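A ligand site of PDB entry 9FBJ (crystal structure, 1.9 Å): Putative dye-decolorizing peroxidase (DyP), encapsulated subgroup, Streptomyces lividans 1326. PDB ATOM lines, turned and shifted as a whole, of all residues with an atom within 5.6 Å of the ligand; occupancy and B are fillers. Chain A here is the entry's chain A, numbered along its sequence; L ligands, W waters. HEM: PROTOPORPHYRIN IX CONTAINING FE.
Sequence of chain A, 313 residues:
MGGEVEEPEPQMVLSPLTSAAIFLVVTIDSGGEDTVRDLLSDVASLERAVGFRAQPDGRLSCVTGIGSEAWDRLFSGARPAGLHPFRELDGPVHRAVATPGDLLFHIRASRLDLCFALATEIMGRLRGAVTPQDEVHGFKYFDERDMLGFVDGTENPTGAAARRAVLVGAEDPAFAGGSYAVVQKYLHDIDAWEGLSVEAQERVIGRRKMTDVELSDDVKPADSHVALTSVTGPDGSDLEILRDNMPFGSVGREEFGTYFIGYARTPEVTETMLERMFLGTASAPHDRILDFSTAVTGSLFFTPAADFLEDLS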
ATOM      1  N   ASP A 146      26.468  23.055 -13.845  1.00  0.00           N
ATOM      2  CA  ASP A 146      27.037  24.059 -12.961  1.00  0.00           C
ATOM      3  C   ASP A 146      28.457  24.267 -13.472  1.00  0.00           C
ATOM      4  O   ASP A 146      28.896  23.600 -14.394  1.00  0.00           O
ATOM      5  CB  ASP A 146      26.831  23.680 -11.522  1.00  0.00           C
ATOM      6  CG  ASP A 146      27.414  22.355 -11.120  1.00  0.00           C
ATOM      7  OD1 ASP A 146      28.411  21.950 -11.732  1.00  0.00           O
ATOM      8  OD2 ASP A 146      26.776  21.671 -10.349  1.00  0.00           O
ATOM      9  N   LEU A 148      31.103  23.270 -12.252  1.00  0.00           N
ATOM     10  CA  LEU A 148      31.936  22.072 -12.077  1.00  0.00           C
ATOM     11  C   LEU A 148      31.728  21.089 -13.242  1.00  0.00           C
ATOM     12  O   LEU A 148      32.440  20.092 -13.390  1.00  0.00           O
ATOM     13  CB  LEU A 148      31.730  21.339 -10.757  1.00  0.00           C
ATOM     14  CG  LEU A 148      31.882  22.139  -9.470  1.00  0.00           C
ATOM     15  CD1 LEU A 148      31.612  21.222  -8.289  1.00  0.00           C
ATOM     16  CD2 LEU A 148      33.266  22.682  -9.374  1.00  0.00           C
ATOM     17  N   PHE A 150      28.822  19.493 -14.066  1.00  0.00           N
ATOM     18  CA  PHE A 150      27.766  18.482 -13.803  1.00  0.00           C
ATOM     19  C   PHE A 150      26.384  19.075 -13.969  1.00  0.00           C
ATOM     20  O   PHE A 150      26.129  20.236 -13.649  1.00  0.00           O
ATOM     21  CB  PHE A 150      27.965  17.872 -12.401  1.00  0.00           C
ATOM     22  CG  PHE A 150      29.084  16.860 -12.325  1.00  0.00           C
ATOM     23  CD1 PHE A 150      30.431  17.276 -12.446  1.00  0.00           C
ATOM     24  CD2 PHE A 150      28.820  15.506 -12.193  1.00  0.00           C
ATOM     25  CE1 PHE A 150      31.438  16.326 -12.404  1.00  0.00           C
ATOM     26  CE2 PHE A 150      29.819  14.570 -12.219  1.00  0.00           C
ATOM     27  CZ  PHE A 150      31.129  14.986 -12.315  1.00  0.00           C
ATOM     28  N   VAL A 151      25.438  18.247 -14.385  1.00  0.00           N
ATOM     29  CA  VAL A 151      24.041  18.643 -14.370  1.00  0.00           C
ATOM     30  C   VAL A 151      23.566  18.898 -12.937  1.00  0.00           C
ATOM     31  O   VAL A 151      23.871  18.129 -12.027  1.00  0.00           O
ATOM     32  CB  VAL A 151      23.175  17.572 -15.079  1.00  0.00           C
ATOM     33  CG1 VAL A 151      21.697  17.943 -14.969  1.00  0.00           C
ATOM     34  CG2 VAL A 151      23.584  17.300 -16.520  1.00  0.00           C
ATOM     35  N   ASP A 152      22.780  19.973 -12.739  1.00  0.00           N
ATOM     36  CA  ASP A 152      22.503  20.491 -11.389  1.00  0.00           C
ATOM     37  C   ASP A 152      20.999  20.736 -11.318  1.00  0.00           C
ATOM     38  O   ASP A 152      20.427  21.474 -12.175  1.00  0.00           O
ATOM     39  CB  ASP A 152      23.396  21.673 -11.056  1.00  0.00           C
ATOM     40  CG  ASP A 152      23.470  22.040  -9.578  1.00  0.00           C
ATOM     41  OD1 ASP A 152      22.427  21.961  -8.932  1.00  0.00           O
ATOM     42  OD2 ASP A 152      24.585  22.351  -9.063  1.00  0.00           O
ATOM     43  N   GLY A 153      20.347  19.908 -10.481  1.00  0.00           N
ATOM     44  CA  GLY A 153      18.904  20.030 -10.244  1.00  0.00           C
ATOM     45  C   GLY A 153      18.123  18.730 -10.456  1.00  0.00           C
ATOM     46  O   GLY A 153      16.938  18.692 -10.132  1.00  0.00           O
ATOM     47  N   THR A 154      18.797  17.667 -10.933  1.00  0.00           N
ATOM     48  CA  THR A 154      18.134  16.445 -11.383  1.00  0.00           C
ATOM     49  C   THR A 154      17.160  15.837 -10.366  1.00  0.00           C
ATOM     50  O   THR A 154      16.082  15.420 -10.757  1.00  0.00           O
ATOM     51  CB  THR A 154      19.222  15.429 -11.696  1.00  0.00           C
ATOM     52  OG1 THR A 154      20.235  16.040 -12.514  1.00  0.00           O
ATOM     53  CG2 THR A 154      18.684  14.236 -12.481  1.00  0.00           C
ATOM     54  N   GLU A 155      17.624  15.612  -9.122  1.00  0.00           N
ATOM     55  CA  GLU A 155      16.849  14.927  -8.101  1.00  0.00           C
ATOM     56  C   GLU A 155      15.961  15.872  -7.290  1.00  0.00           C
ATOM     57  O   GLU A 155      15.342  15.423  -6.341  1.00  0.00           O
ATOM     58  CB  GLU A 155      17.769  14.071  -7.175  1.00  0.00           C
ATOM     59  CG  GLU A 155      18.289  12.813  -7.889  1.00  0.00           C
ATOM     60  CD  GLU A 155      17.206  11.961  -8.478  1.00  0.00           C
ATOM     61  OE1 GLU A 155      16.549  11.473  -7.585  1.00  0.00           O
ATOM     62  OE2 GLU A 155      16.837  11.969  -9.673  1.00  0.00           O
ATOM     63  N   ASN A 156      15.744  17.128  -7.729  1.00  0.00           N
ATOM     64  CA  ASN A 156      14.785  18.026  -7.098  1.00  0.00           C
ATOM     65  C   ASN A 156      13.399  17.347  -7.089  1.00  0.00           C
ATOM     66  O   ASN A 156      13.025  16.655  -8.035  1.00  0.00           O
ATOM     67  CB  ASN A 156      14.645  19.370  -7.810  1.00  0.00           C
ATOM     68  CG  ASN A 156      15.503  20.503  -7.262  1.00  0.00           C
ATOM     69  OD1 ASN A 156      15.796  20.554  -6.072  1.00  0.00           O
ATOM     70  ND2 ASN A 156      15.918  21.426  -8.148  1.00  0.00           N
ATOM     71  N   GLN A 184      23.760  30.319   0.254  1.00  0.00           N
ATOM     72  CA  GLN A 184      25.206  30.453   0.360  1.00  0.00           C
ATOM     73  C   GLN A 184      25.814  30.723  -1.013  1.00  0.00           C
ATOM     74  O   GLN A 184      25.626  29.911  -1.920  1.00  0.00           O
ATOM     75  CB  GLN A 184      25.921  29.234   0.926  1.00  0.00           C
ATOM     76  CG  GLN A 184      25.494  28.689   2.291  1.00  0.00           C
ATOM     77  CD  GLN A 184      26.089  27.330   2.591  1.00  0.00           C
ATOM     78  OE1 GLN A 184      25.778  26.300   1.984  1.00  0.00           O
ATOM     79  NE2 GLN A 184      27.028  27.321   3.540  1.00  0.00           N
ATOM     80  N   TYR A 186      29.096  30.138  -3.135  1.00  0.00           N
ATOM     81  CA  TYR A 186      30.308  29.362  -3.143  1.00  0.00           C
ATOM     82  C   TYR A 186      31.183  29.824  -4.319  1.00  0.00           C
ATOM     83  O   TYR A 186      30.645  30.298  -5.340  1.00  0.00           O
ATOM     84  CB  TYR A 186      30.020  27.882  -3.376  1.00  0.00           C
ATOM     85  CG  TYR A 186      29.430  27.134  -2.191  1.00  0.00           C
ATOM     86  CD1 TYR A 186      30.293  26.535  -1.259  1.00  0.00           C
ATOM     87  CD2 TYR A 186      28.075  27.037  -1.985  1.00  0.00           C
ATOM     88  CE1 TYR A 186      29.810  25.887  -0.164  1.00  0.00           C
ATOM     89  CE2 TYR A 186      27.572  26.370  -0.903  1.00  0.00           C
ATOM     90  CZ  TYR A 186      28.450  25.768   0.003  1.00  0.00           C
ATOM     91  OH  TYR A 186      28.058  25.020   1.064  1.00  0.00           O
ATOM     92  N   HIS A 188      34.550  28.367  -6.556  1.00  0.00           N
ATOM     93  CA  HIS A 188      35.202  27.111  -6.925  1.00  0.00           C
ATOM     94  C   HIS A 188      36.667  27.296  -7.316  1.00  0.00           C
ATOM     95  O   HIS A 188      37.007  28.263  -7.951  1.00  0.00           O
ATOM     96  CB  HIS A 188      34.449  26.495  -8.072  1.00  0.00           C
ATOM     97  CG  HIS A 188      33.062  26.089  -7.678  1.00  0.00           C
ATOM     98  ND1 HIS A 188      32.825  25.134  -6.701  1.00  0.00           N
ATOM     99  CD2 HIS A 188      31.874  26.411  -8.210  1.00  0.00           C
ATOM    100  CE1 HIS A 188      31.525  24.984  -6.597  1.00  0.00           C
ATOM    101  NE2 HIS A 188      30.915  25.681  -7.540  1.00  0.00           N
ATOM    102  N   ILE A 205      31.171  13.755  -6.718  1.00  0.00           N
ATOM    103  CA  ILE A 205      29.765  14.171  -6.795  1.00  0.00           C
ATOM    104  C   ILE A 205      28.887  12.988  -6.395  1.00  0.00           C
ATOM    105  O   ILE A 205      27.829  13.199  -5.777  1.00  0.00           O
ATOM    106  CB  ILE A 205      29.375  14.656  -8.206  1.00  0.00           C
ATOM    107  CG1 ILE A 205      30.240  15.864  -8.704  1.00  0.00           C
ATOM    108  CG2 ILE A 205      27.868  14.887  -8.311  1.00  0.00           C
ATOM    109  CD1 ILE A 205      30.100  17.076  -7.811  1.00  0.00           C
ATOM    110  N   ARG A 207      27.578  10.866  -9.232  1.00  0.00           N
ATOM    111  CA  ARG A 207      26.887  10.695 -10.507  1.00  0.00           C
ATOM    112  C   ARG A 207      27.886  10.761 -11.678  1.00  0.00           C
ATOM    113  O   ARG A 207      28.930  11.416 -11.576  1.00  0.00           O
ATOM    114  CB  ARG A 207      25.861  11.814 -10.700  1.00  0.00           C
ATOM    115  CG  ARG A 207      24.834  11.969  -9.553  1.00  0.00           C
ATOM    116  CD  ARG A 207      23.779  13.011  -9.849  1.00  0.00           C
ATOM    117  NE  ARG A 207      22.782  12.492 -10.759  1.00  0.00           N
ATOM    118  CZ  ARG A 207      21.699  11.811 -10.416  1.00  0.00           C
ATOM    119  NH1 ARG A 207      21.427  11.547  -9.133  1.00  0.00           N
ATOM    120  NH2 ARG A 207      20.934  11.315 -11.360  1.00  0.00           N
ATOM    121  N   ASP A 212      24.741  11.777 -16.363  1.00  0.00           N
ATOM    122  CA  ASP A 212      24.028  12.168 -15.146  1.00  0.00           C
ATOM    123  C   ASP A 212      23.283  10.988 -14.516  1.00  0.00           C
ATOM    124  O   ASP A 212      22.281  11.182 -13.864  1.00  0.00           O
ATOM    125  CB  ASP A 212      23.009  13.224 -15.485  1.00  0.00           C
ATOM    126  CG  ASP A 212      22.460  13.955 -14.260  1.00  0.00           C
ATOM    127  OD1 ASP A 212      23.038  13.826 -13.212  1.00  0.00           O
ATOM    128  OD2 ASP A 212      21.448  14.639 -14.357  1.00  0.00           O
ATOM    129  N   GLU A 214      23.112   8.128 -11.746  1.00  0.00           N
ATOM    130  CA  GLU A 214      23.615   7.859 -10.391  1.00  0.00           C
ATOM    131  C   GLU A 214      24.510   6.627 -10.339  1.00  0.00           C
ATOM    132  O   GLU A 214      24.280   5.616 -10.988  1.00  0.00           O
ATOM    133  CB  GLU A 214      22.438   7.869  -9.380  1.00  0.00           C
ATOM    134  CG  GLU A 214      22.839   7.605  -7.922  1.00  0.00           C
ATOM    135  CD  GLU A 214      21.722   7.734  -6.856  1.00  0.00           C
ATOM    136  OE1 GLU A 214      20.556   7.916  -7.192  1.00  0.00           O
ATOM    137  OE2 GLU A 214      22.025   7.748  -5.685  1.00  0.00           O
ATOM    138  N   HIS A 225      29.090  13.853  -2.561  1.00  0.00           N
ATOM    139  CA  HIS A 225      28.067  14.838  -2.359  1.00  0.00           C
ATOM    140  C   HIS A 225      26.687  14.214  -2.176  1.00  0.00           C
ATOM    141  O   HIS A 225      25.926  14.622  -1.279  1.00  0.00           O
ATOM    142  CB  HIS A 225      28.098  15.906  -3.437  1.00  0.00           C
ATOM    143  CG  HIS A 225      27.186  17.035  -3.169  1.00  0.00           C
ATOM    144  ND1 HIS A 225      27.195  17.780  -2.016  1.00  0.00           N
ATOM    145  CD2 HIS A 225      26.200  17.583  -3.995  1.00  0.00           C
ATOM    146  CE1 HIS A 225      26.226  18.726  -2.144  1.00  0.00           C
ATOM    147  NE2 HIS A 225      25.608  18.638  -3.314  1.00  0.00           N
ATOM    148  N   VAL A 226      26.374  13.288  -3.060  1.00  0.00           N
ATOM    149  CA  VAL A 226      25.040  12.739  -3.124  1.00  0.00           C
ATOM    150  C   VAL A 226      24.783  11.856  -1.900  1.00  0.00           C
ATOM    151  O   VAL A 226      23.649  11.717  -1.471  1.00  0.00           O
ATOM    152  CB  VAL A 226      24.813  12.001  -4.470  1.00  0.00           C
ATOM    153  CG1 VAL A 226      23.661  10.942  -4.425  1.00  0.00           C
ATOM    154  CG2 VAL A 226      24.562  12.999  -5.610  1.00  0.00           C
ATOM    155  N   THR A 229      24.115  14.244   1.198  1.00  0.00           N
ATOM    156  CA  THR A 229      22.915  15.077   1.153  1.00  0.00           C
ATOM    157  C   THR A 229      21.669  14.185   0.972  1.00  0.00           C
ATOM    158  O   THR A 229      20.592  14.707   0.726  1.00  0.00           O
ATOM    159  CB  THR A 229      23.005  16.149   0.050  1.00  0.00           C
ATOM    160  OG1 THR A 229      23.308  15.504  -1.168  1.00  0.00           O
ATOM    161  CG2 THR A 229      24.168  17.113   0.254  1.00  0.00           C
ATOM    162  N   SER A 230      21.827  12.838   0.997  1.00  0.00           N
ATOM    163  CA  SER A 230      20.707  11.894   1.113  1.00  0.00           C
ATOM    164  C   SER A 230      20.449  11.557   2.588  1.00  0.00           C
ATOM    165  O   SER A 230      21.297  10.987   3.271  1.00  0.00           O
ATOM    166  CB  SER A 230      20.919  10.588   0.386  1.00  0.00           C
ATOM    167  OG  SER A 230      21.426  10.848  -0.896  1.00  0.00           O
ATOM    168  N   ILE A 241      14.699  18.765  -0.135  1.00  0.00           N
ATOM    169  CA  ILE A 241      14.633  20.199  -0.332  1.00  0.00           C
ATOM    170  C   ILE A 241      14.538  20.515  -1.814  1.00  0.00           C
ATOM    171  O   ILE A 241      14.765  19.664  -2.659  1.00  0.00           O
ATOM    172  CB  ILE A 241      15.836  20.923   0.295  1.00  0.00           C
ATOM    173  CG1 ILE A 241      17.136  20.690  -0.508  1.00  0.00           C
ATOM    174  CG2 ILE A 241      16.028  20.553   1.783  1.00  0.00           C
ATOM    175  CD1 ILE A 241      18.318  21.472   0.075  1.00  0.00           C
ATOM    176  N   ARG A 243      16.155  22.948  -4.599  1.00  0.00           N
ATOM    177  CA  ARG A 243      17.273  23.817  -4.962  1.00  0.00           C
ATOM    178  C   ARG A 243      17.040  24.507  -6.327  1.00  0.00           C
ATOM    179  O   ARG A 243      16.379  23.996  -7.200  1.00  0.00           O
ATOM    180  CB  ARG A 243      18.541  22.963  -5.007  1.00  0.00           C
ATOM    181  CG  ARG A 243      18.903  22.227  -3.723  1.00  0.00           C
ATOM    182  CD  ARG A 243      19.846  21.062  -3.924  1.00  0.00           C
ATOM    183  NE  ARG A 243      19.182  20.011  -4.718  1.00  0.00           N
ATOM    184  CZ  ARG A 243      19.602  19.537  -5.886  1.00  0.00           C
ATOM    185  NH1 ARG A 243      20.669  20.021  -6.535  1.00  0.00           N
ATOM    186  NH2 ARG A 243      18.907  18.570  -6.419  1.00  0.00           N
ATOM    187  N   ASN A 245      20.062  26.259  -7.746  1.00  0.00           N
ATOM    188  CA  ASN A 245      21.449  26.651  -7.912  1.00  0.00           C
ATOM    189  C   ASN A 245      21.716  27.342  -9.247  1.00  0.00           C
ATOM    190  O   ASN A 245      21.381  26.786 -10.294  1.00  0.00           O
ATOM    191  CB  ASN A 245      22.340  25.444  -7.812  1.00  0.00           C
ATOM    192  CG  ASN A 245      22.318  24.804  -6.445  1.00  0.00           C
ATOM    193  OD1 ASN A 245      21.697  25.306  -5.496  1.00  0.00           O
ATOM    194  ND2 ASN A 245      23.003  23.688  -6.320  1.00  0.00           N
ATOM    195  N   THR A 258      29.007  29.037  -7.800  1.00  0.00           N
ATOM    196  CA  THR A 258      27.628  28.557  -7.716  1.00  0.00           C
ATOM    197  C   THR A 258      26.977  29.319  -6.566  1.00  0.00           C
ATOM    198  O   THR A 258      27.462  29.300  -5.446  1.00  0.00           O
ATOM    199  CB  THR A 258      27.605  27.063  -7.427  1.00  0.00           C
ATOM    200  OG1 THR A 258      28.260  26.281  -8.439  1.00  0.00           O
ATOM    201  CG2 THR A 258      26.179  26.544  -7.239  1.00  0.00           C
ATOM    202  N   PHE A 260      24.141  28.804  -4.254  1.00  0.00           N
ATOM    203  CA  PHE A 260      23.211  27.844  -3.693  1.00  0.00           C
ATOM    204  C   PHE A 260      21.976  28.512  -3.084  1.00  0.00           C
ATOM    205  O   PHE A 260      22.028  29.503  -2.379  1.00  0.00           O
ATOM    206  CB  PHE A 260      23.970  26.989  -2.669  1.00  0.00           C
ATOM    207  CG  PHE A 260      23.021  26.099  -1.892  1.00  0.00           C
ATOM    208  CD1 PHE A 260      22.625  24.877  -2.403  1.00  0.00           C
ATOM    209  CD2 PHE A 260      22.517  26.482  -0.658  1.00  0.00           C
ATOM    210  CE1 PHE A 260      21.722  24.053  -1.669  1.00  0.00           C
ATOM    211  CE2 PHE A 260      21.626  25.640   0.055  1.00  0.00           C
ATOM    212  CZ  PHE A 260      21.216  24.457  -0.476  1.00  0.00           C
ATOM    213  N   THR A 270      17.424  21.357   5.920  1.00  0.00           N
ATOM    214  CA  THR A 270      18.607  21.947   5.305  1.00  0.00           C
ATOM    215  C   THR A 270      19.829  21.846   6.245  1.00  0.00           C
ATOM    216  O   THR A 270      20.921  21.590   5.754  1.00  0.00           O
ATOM    217  CB  THR A 270      18.270  23.358   4.860  1.00  0.00           C
ATOM    218  OG1 THR A 270      17.020  23.284   4.182  1.00  0.00           O
ATOM    219  CG2 THR A 270      19.361  24.004   4.011  1.00  0.00           C
ATOM    220  N   MET A 273      21.528  18.500   6.518  1.00  0.00           N
ATOM    221  CA  MET A 273      22.414  18.253   5.379  1.00  0.00           C
ATOM    222  C   MET A 273      23.675  19.120   5.418  1.00  0.00           C
ATOM    223  O   MET A 273      24.728  18.600   5.025  1.00  0.00           O
ATOM    224  CB  MET A 273      21.677  18.609   4.064  1.00  0.00           C
ATOM    225  CG  MET A 273      20.478  17.773   3.708  1.00  0.00           C
ATOM    226  SD  MET A 273      19.602  18.494   2.281  1.00  0.00           S
ATOM    227  CE  MET A 273      18.430  17.230   1.820  1.00  0.00           C
ATOM    228  N   LEU A 274      23.652  20.357   6.009  1.00  0.00           N
ATOM    229  CA  LEU A 274      24.851  21.174   6.099  1.00  0.00           C
ATOM    230  C   LEU A 274      25.774  20.576   7.187  1.00  0.00           C
ATOM    231  O   LEU A 274      26.984  20.625   7.063  1.00  0.00           O
ATOM    232  CB  LEU A 274      24.591  22.660   6.397  1.00  0.00           C
ATOM    233  CG  LEU A 274      23.850  23.455   5.291  1.00  0.00           C
ATOM    234  CD1 LEU A 274      23.217  24.771   5.717  1.00  0.00           C
ATOM    235  CD2 LEU A 274      24.912  23.715   4.210  1.00  0.00           C
ATOM    236  N   MET A 277      27.721  17.684   5.610  1.00  0.00           N
ATOM    237  CA  MET A 277      28.762  18.168   4.713  1.00  0.00           C
ATOM    238  C   MET A 277      29.989  18.729   5.421  1.00  0.00           C
ATOM    239  O   MET A 277      31.130  18.426   5.031  1.00  0.00           O
ATOM    240  CB  MET A 277      28.168  19.287   3.826  1.00  0.00           C
ATOM    241  CG  MET A 277      27.055  18.790   2.914  1.00  0.00           C
ATOM    242  SD  MET A 277      26.358  20.046   1.801  1.00  0.00           S
ATOM    243  CE  MET A 277      27.881  20.768   1.166  1.00  0.00           C
ATOM    244  N   ILE A 289      33.003  17.703  -2.019  1.00  0.00           N
ATOM    245  CA  ILE A 289      32.722  18.867  -2.855  1.00  0.00           C
ATOM    246  C   ILE A 289      33.291  20.152  -2.211  1.00  0.00           C
ATOM    247  O   ILE A 289      33.728  21.056  -2.942  1.00  0.00           O
ATOM    248  CB  ILE A 289      31.212  18.926  -3.231  1.00  0.00           C
ATOM    249  CG1 ILE A 289      31.059  19.683  -4.550  1.00  0.00           C
ATOM    250  CG2 ILE A 289      30.332  19.594  -2.183  1.00  0.00           C
ATOM    251  CD1 ILE A 289      29.636  19.661  -5.099  1.00  0.00           C
ATOM    252  N   SER A 293      35.340  23.993  -3.078  1.00  0.00           N
ATOM    253  CA  SER A 293      34.268  24.973  -3.040  1.00  0.00           C
ATOM    254  C   SER A 293      34.346  25.640  -1.680  1.00  0.00           C
ATOM    255  O   SER A 293      34.271  24.924  -0.665  1.00  0.00           O
ATOM    256  CB  SER A 293      32.886  24.335  -3.244  1.00  0.00           C
ATOM    257  OG  SER A 293      32.911  23.416  -4.331  1.00  0.00           O
HETATM  258  CHA HEM L   1      22.651  17.247  -5.392  1.00  0.00           C
HETATM  259  CHB HEM L   1      26.008  20.307  -6.872  1.00  0.00           C
HETATM  260  CHC HEM L   1      25.740  22.488  -2.613  1.00  0.00           C
HETATM  261  CHD HEM L   1      22.120  19.806  -1.431  1.00  0.00           C
HETATM  262  C1A HEM L   1      23.595  17.873  -6.194  1.00  0.00           C
HETATM  263  C2A HEM L   1      24.010  17.420  -7.470  1.00  0.00           C
HETATM  264  C3A HEM L   1      24.996  18.269  -7.866  1.00  0.00           C
HETATM  265  C4A HEM L   1      25.119  19.266  -6.815  1.00  0.00           C
HETATM  266  CMA HEM L   1      25.808  18.370  -9.149  1.00  0.00           C
HETATM  267  CAA HEM L   1      23.500  16.164  -8.317  1.00  0.00           C
HETATM  268  CBA HEM L   1      22.419  16.618  -9.351  1.00  0.00           C
HETATM  269  CGA HEM L   1      21.130  16.891  -8.627  1.00  0.00           C
HETATM  270  O1A HEM L   1      20.994  18.077  -8.301  1.00  0.00           O
HETATM  271  O2A HEM L   1      20.353  15.957  -8.182  1.00  0.00           O
HETATM  272  C1B HEM L   1      26.198  21.222  -5.867  1.00  0.00           C
HETATM  273  C2B HEM L   1      27.235  22.195  -5.891  1.00  0.00           C
HETATM  274  C3B HEM L   1      27.131  22.866  -4.668  1.00  0.00           C
HETATM  275  C4B HEM L   1      26.123  22.190  -3.912  1.00  0.00           C
HETATM  276  CMB HEM L   1      28.127  22.659  -7.049  1.00  0.00           C
HETATM  277  CAB HEM L   1      28.112  23.941  -4.443  1.00  0.00           C
HETATM  278  CBB HEM L   1      28.603  24.332  -3.338  1.00  0.00           C
HETATM  279  C1C HEM L   1      24.740  21.964  -1.869  1.00  0.00           C
HETATM  280  C2C HEM L   1      24.252  22.422  -0.595  1.00  0.00           C
HETATM  281  C3C HEM L   1      23.200  21.632  -0.238  1.00  0.00           C
HETATM  282  C4C HEM L   1      23.063  20.712  -1.324  1.00  0.00           C
HETATM  283  CMC HEM L   1      24.878  23.496   0.340  1.00  0.00           C
HETATM  284  CAC HEM L   1      22.289  21.515   0.949  1.00  0.00           C
HETATM  285  CBC HEM L   1      22.336  22.188   2.053  1.00  0.00           C
HETATM  286  C1D HEM L   1      21.983  18.913  -2.485  1.00  0.00           C
HETATM  287  C2D HEM L   1      20.896  17.849  -2.517  1.00  0.00           C
HETATM  288  C3D HEM L   1      21.112  17.080  -3.564  1.00  0.00           C
HETATM  289  C4D HEM L   1      22.257  17.728  -4.210  1.00  0.00           C
HETATM  290  CMD HEM L   1      19.813  17.507  -1.436  1.00  0.00           C
HETATM  291  CAD HEM L   1      20.304  15.903  -4.065  1.00  0.00           C
HETATM  292  CBD HEM L   1      20.808  14.632  -3.472  1.00  0.00           C
HETATM  293  CGD HEM L   1      19.992  13.363  -3.891  1.00  0.00           C
HETATM  294  O1D HEM L   1      19.038  13.104  -3.165  1.00  0.00           O
HETATM  295  O2D HEM L   1      20.240  12.697  -4.916  1.00  0.00           O
HETATM  296  NA  HEM L   1      24.348  18.925  -5.741  1.00  0.00           N
HETATM  297  NB  HEM L   1      25.694  21.200  -4.689  1.00  0.00           N
HETATM  298  NC  HEM L   1      23.991  20.971  -2.299  1.00  0.00           N
HETATM  299  ND  HEM L   1      22.742  18.791  -3.563  1.00  0.00           N
HETATM  300 FE   HEM L   1      24.173  19.918  -4.078  1.00  0.00          FE
HETATM  301  O   HOH W   1      21.552  13.560  -7.143  1.00  0.00           O
HETATM  302  O   HOH W   2      18.326  14.500  -1.059  1.00  0.00           O
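Asp 146 touches the ligand (OD2 to CMA, 3.6 Å).
Leu 148 touches the ligand.
CB of Phe 150 touches CMA of the ligand, at 3.9 Å.
Val 151 touches the ligand.
Asp 152 touches the ligand.
Gln 184 touches the ligand (OE1 to CMC, 3.4 Å).
Tyr 186 touches the ligand (CD2 to CBB, 3.1 Å).
CD of Arg 207 touches CAA of the ligand (3.5 Å).
Val 226 touches the ligand (CG1 to O2D, 3.9 Å).
Thr 229 touches the ligand (OG1 to CBD, 3.5 Å).
Ser 230 touches the ligand (OG to O1D, 3.99 Å).
Thr 258 touches the ligand.
Phe 260 touches the ligand.
Thr 270 touches the ligand.
CE of Met 273 touches CMD of the ligand, 3.5 Å away.
Leu 274 touches the ligand.
Met 277 touches the ligand.
CD1 of Ile 289 touches C2B of the ligand (3.6 Å).
Hydrophobic or aromatic side chains that line the ligand: Leu 148, Phe 150, Tyr 186, His 225, Val 226, Phe 260, Met 273, Leu 274, Met 277 and Ile 289.
23 residues have an atom within 4 Å of the ligand: Asp 146, Leu 148, Phe 150, Val 151, Asp 152, Gly 153, Thr 154, Glu 155, Gln 184, Tyr 186, Arg 207, His 225, Val 226, Thr 229, Ser 230, Arg 243, Thr 258, Phe 260, Thr 270, Met 273, Leu 274, Met 277 and Ile 289.
Along chain A the residues within 4 Å of the ligand span positions 146 to 289.
N of Thr 154 lies close to O1A of the ligand (3.5 Å).
O1A of the ligand lies within hydrogen-bond range of N of Gly 153, 2.9 Å away.
A ring nitrogen (NE2) of His 225 is bound to an iron atom (FE) of the ligand (2.1 Å).
An oxygen (O1A) of the ligand lies within salt-bridge range of the guanidinium group of Arg 243, at 2.6 Å.
The backbone NH of Glu 155 lies within hydrogen-bond range of an oxygen (O2A) of the ligand (2.9 Å).
Water W2 bridges an oxygen (O1D) of the ligand (2.6 Å) and the backbone carbonyl oxygen of Thr 229 (2.9 Å).
Water W1 lies within hydrogen-bond range of O2D of the ligand (2.7 Å) and NH1 of Arg 207 (2.8 Å).
OD1 of Asp 152 is in hydrogen-bond range of ND2 of Asn 245 (3.2 Å).
The backbone NH (N) of Phe 150 sits at hydrogen-bond distance from the side-chain carboxylate (OD1) of Asp 146 (3.4 Å).
The side-chain hydroxyl (OH) of Tyr 186 sits at hydrogen-bond distance from the side-chain amide oxygen (OE1) of Gln 184.
NE of Arg 207 is in salt-bridge range of OD1 of Asp 212 (2.8 Å).
OD2 of Asp 152 sits close to OD2 of Asp 146 (2.6 Å).
The side-chain hydroxyl of Thr 154 sits at hydrogen-bond distance from the side-chain carboxylate of Asp 212 (2.6 Å).
A ring nitrogen (NE2) of His 188 sits at hydrogen-bond distance from the side-chain hydroxyl of Thr 258, 2.9 Å away.
The backbone carbonyl oxygen (O) of Arg 243 is in hydrogen-bond range of the side-chain amide nitrogen (ND2) of Asn 156 (2.8 Å).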
